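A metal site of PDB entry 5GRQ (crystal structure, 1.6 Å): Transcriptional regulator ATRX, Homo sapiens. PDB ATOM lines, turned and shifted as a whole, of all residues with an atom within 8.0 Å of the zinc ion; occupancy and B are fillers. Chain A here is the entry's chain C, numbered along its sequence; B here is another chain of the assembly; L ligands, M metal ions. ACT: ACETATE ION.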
ATOM      1  N   VAL A   3     -28.548  -6.552  11.882  1.00  0.00           N
ATOM      2  CA  VAL A   3     -28.036  -7.794  12.447  1.00  0.00           C
ATOM      3  C   VAL A   3     -28.742  -8.957  11.778  1.00  0.00           C
ATOM      4  O   VAL A   3     -29.835  -8.827  11.229  1.00  0.00           O
ATOM      5  CB  VAL A   3     -28.223  -7.859  13.987  1.00  0.00           C
ATOM      6  CG1 VAL A   3     -27.555  -6.671  14.652  1.00  0.00           C
ATOM      7  CG2 VAL A   3     -29.696  -7.942  14.342  1.00  0.00           C
ATOM      8  N   ASP A   4     -28.103 -10.125  11.825  1.00  0.00           N
ATOM      9  CA  ASP A   4     -28.752 -11.331  11.304  1.00  0.00           C
ATOM     10  C   ASP A   4     -28.848 -12.382  12.413  1.00  0.00           C
ATOM     11  O   ASP A   4     -28.661 -12.093  13.606  1.00  0.00           O
ATOM     12  CB  ASP A   4     -28.046 -11.859  10.046  1.00  0.00           C
ATOM     13  CG  ASP A   4     -26.630 -12.392  10.297  1.00  0.00           C
ATOM     14  OD1 ASP A   4     -26.217 -12.604  11.457  1.00  0.00           O
ATOM     15  OD2 ASP A   4     -25.931 -12.599   9.287  1.00  0.00           O
ATOM     16  N   ASP A   5     -29.172 -13.612  12.013  1.00  0.00           N
ATOM     17  CA  ASP A   5     -29.539 -14.621  12.989  1.00  0.00           C
ATOM     18  C   ASP A   5     -28.351 -15.180  13.758  1.00  0.00           C
ATOM     19  O   ASP A   5     -28.555 -15.738  14.844  1.00  0.00           O
ATOM     20  CB  ASP A   5     -30.263 -15.797  12.314  1.00  0.00           C
ATOM     21  CG  ASP A   5     -31.704 -15.489  11.957  1.00  0.00           C
ATOM     22  OD1 ASP A   5     -32.202 -14.394  12.310  1.00  0.00           O
ATOM     23  OD2 ASP A   5     -32.347 -16.354  11.324  1.00  0.00           O
ATOM     24  N   ASP A   6     -27.128 -15.063  13.246  1.00  0.00           N
ATOM     25  CA  ASP A   6     -25.984 -15.787  13.790  1.00  0.00           C
ATOM     26  C   ASP A   6     -25.050 -14.858  14.549  1.00  0.00           C
ATOM     27  O   ASP A   6     -25.198 -13.622  14.529  1.00  0.00           O
ATOM     28  CB  ASP A   6     -25.226 -16.517  12.672  1.00  0.00           C
ATOM     29  CG  ASP A   6     -24.464 -15.582  11.756  1.00  0.00           C
ATOM     30  OD1 ASP A   6     -23.366 -15.119  12.121  1.00  0.00           O
ATOM     31  OD2 ASP A   6     -24.980 -15.305  10.655  1.00  0.00           O
ATOM     32  N   ASP A   7     -24.050 -15.461  15.215  1.00  0.00           N
ATOM     33  CA  ASP A   7     -23.027 -14.714  15.953  1.00  0.00           C
ATOM     34  C   ASP A   7     -21.613 -15.037  15.477  1.00  0.00           C
ATOM     35  O   ASP A   7     -20.663 -14.977  16.258  1.00  0.00           O
ATOM     36  CB  ASP A   7     -23.169 -14.955  17.457  1.00  0.00           C
ATOM     37  CG  ASP A   7     -23.107 -16.421  17.832  1.00  0.00           C
ATOM     38  OD1 ASP A   7     -22.927 -17.268  16.936  1.00  0.00           O
ATOM     39  OD2 ASP A   7     -23.262 -16.726  19.028  1.00  0.00           O
ATOM     40  N   ASP A   8     -21.462 -15.358  14.196  1.00  0.00           N
ATOM     41  CA  ASP A   8     -20.168 -15.740  13.637  1.00  0.00           C
ATOM     42  C   ASP A   8     -19.481 -14.620  12.845  1.00  0.00           C
ATOM     43  O   ASP A   8     -18.383 -14.849  12.337  1.00  0.00           O
ATOM     44  CB  ASP A   8     -20.346 -16.956  12.720  1.00  0.00           C
ATOM     45  CG  ASP A   8     -20.881 -18.169  13.465  1.00  0.00           C
ATOM     46  OD1 ASP A   8     -20.342 -18.499  14.544  1.00  0.00           O
ATOM     47  OD2 ASP A   8     -21.864 -18.759  12.975  1.00  0.00           O
ATOM     48  N   ASP A   9     -20.078 -13.426  12.762  1.00  0.00           N
ATOM     49  CA  ASP A   9     -19.695 -12.418  11.788  1.00  0.00           C
ATOM     50  C   ASP A   9     -18.720 -11.364  12.289  1.00  0.00           C
ATOM     51  O   ASP A   9     -18.246 -10.553  11.481  1.00  0.00           O
ATOM     52  CB  ASP A   9     -20.945 -11.708  11.247  1.00  0.00           C
ATOM     53  CG  ASP A   9     -21.866 -12.658  10.510  1.00  0.00           C
ATOM     54  OD1 ASP A   9     -21.355 -13.636   9.927  1.00  0.00           O
ATOM     55  OD2 ASP A   9     -23.104 -12.431  10.526  1.00  0.00           O
ATOM     56  N   ASN A  10     -18.409 -11.329  13.593  1.00  0.00           N
ATOM     57  CA  ASN A  10     -17.568 -10.243  14.099  1.00  0.00           C
ATOM     58  C   ASN A  10     -16.190 -10.237  13.435  1.00  0.00           C
ATOM     59  O   ASN A  10     -15.669  -9.167  13.115  1.00  0.00           O
ATOM     60  CB  ASN A  10     -17.428 -10.349  15.624  1.00  0.00           C
ATOM     61  CG  ASN A  10     -18.649  -9.838  16.352  1.00  0.00           C
ATOM     62  OD1 ASN A  10     -19.333  -8.919  15.882  1.00  0.00           O
ATOM     63  ND2 ASN A  10     -18.952 -10.422  17.504  1.00  0.00           N
ATOM     64  N   ARG A  15     -15.926 -15.232   8.999  1.00  0.00           N
ATOM     65  CA  ARG A  15     -17.097 -15.207   8.134  1.00  0.00           C
ATOM     66  C   ARG A  15     -16.783 -15.850   6.778  1.00  0.00           C
ATOM     67  O   ARG A  15     -17.591 -16.615   6.240  1.00  0.00           O
ATOM     68  CB  ARG A  15     -17.570 -13.765   7.960  1.00  0.00           C
ATOM     69  CG  ARG A  15     -18.953 -13.640   7.359  1.00  0.00           C
ATOM     70  CD  ARG A  15     -19.491 -12.213   7.421  1.00  0.00           C
ATOM     71  NE  ARG A  15     -20.833 -12.144   6.874  1.00  0.00           N
ATOM     72  CZ  ARG A  15     -21.643 -11.092   6.971  1.00  0.00           C
ATOM     73  NH1 ARG A  15     -21.237 -10.002   7.618  1.00  0.00           N
ATOM     74  NH2 ARG A  15     -22.855 -11.134   6.438  1.00  0.00           N
ATOM     75  N   LYS A  18     -16.236 -19.706   7.294  1.00  0.00           N
ATOM     76  CA  LYS A  18     -17.517 -20.373   7.484  1.00  0.00           C
ATOM     77  C   LYS A  18     -18.245 -20.561   6.162  1.00  0.00           C
ATOM     78  O   LYS A  18     -18.756 -21.652   5.874  1.00  0.00           O
ATOM     79  CB  LYS A  18     -18.378 -19.564   8.462  1.00  0.00           C
ATOM     80  CG  LYS A  18     -19.768 -20.128   8.688  1.00  0.00           C
ATOM     81  CD  LYS A  18     -20.551 -19.243   9.651  1.00  0.00           C
ATOM     82  CE  LYS A  18     -22.002 -19.647   9.731  1.00  0.00           C
ATOM     83  NZ  LYS A  18     -22.836 -18.591  10.445  1.00  0.00           N
ATOM     84  N   ASP B  26     -26.382 -24.254  14.888  1.00  0.00           N
ATOM     85  CA  ASP B  26     -27.172 -23.788  13.754  1.00  0.00           C
ATOM     86  C   ASP B  26     -26.730 -24.413  12.447  1.00  0.00           C
ATOM     87  O   ASP B  26     -27.408 -24.195  11.426  1.00  0.00           O
ATOM     88  CB  ASP B  26     -27.152 -22.250  13.658  1.00  0.00           C
ATOM     89  CG  ASP B  26     -25.764 -21.612  13.802  1.00  0.00           C
ATOM     90  OD1 ASP B  26     -24.754 -22.305  14.074  1.00  0.00           O
ATOM     91  OD2 ASP B  26     -25.690 -20.364  13.633  1.00  0.00           O
HETATM   92  C   ACT L   1     -24.050 -14.587   7.062  1.00  0.00           C
HETATM   93  O   ACT L   1     -23.409 -13.591   7.498  1.00  0.00           O
HETATM   94  OXT ACT L   1     -24.927 -15.284   7.640  1.00  0.00           O
HETATM   95  CH3 ACT L   1     -23.702 -15.007   5.587  1.00  0.00           C
HETATM   96 ZN    ZN M   1     -24.291 -13.697   9.614  1.00  0.00          ZN
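The zinc ion is bound by the side-chain carboxylate (OD2) of Asp 9 (2.0 Å), the side-chain carboxylate (OD2) of Asp 4 (2.0 Å), the side-chain carboxylate (OD2) of Asp 6 (2.0 Å) and an oxygen (O) of the ligand (2.3 Å). The zinc ion has four donor atoms within binding distance. Slightly farther from the zinc ion lies an oxygen (OXT) of the ligand (2.6 Å).
Along chain A the residues within 4 Å of the zinc ion span positions 4 to 9. The nearest printed residue that does not touch the zinc ion is Arg 15 (4.3 Å).
The guanidinium group (NE) of Arg 15 is in salt-bridge range of the side-chain carboxylate (OD1) of Asp 9 (3.4 Å). The side-chain carboxylate (OD1) of Asp 6 lies within salt-bridge range of the side-chain amino group (NZ) of Lys 18. The side-chain carboxylate of Asp 6 is in hydrogen-bond range of the backbone NH of Asp 8 (2.8 Å).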
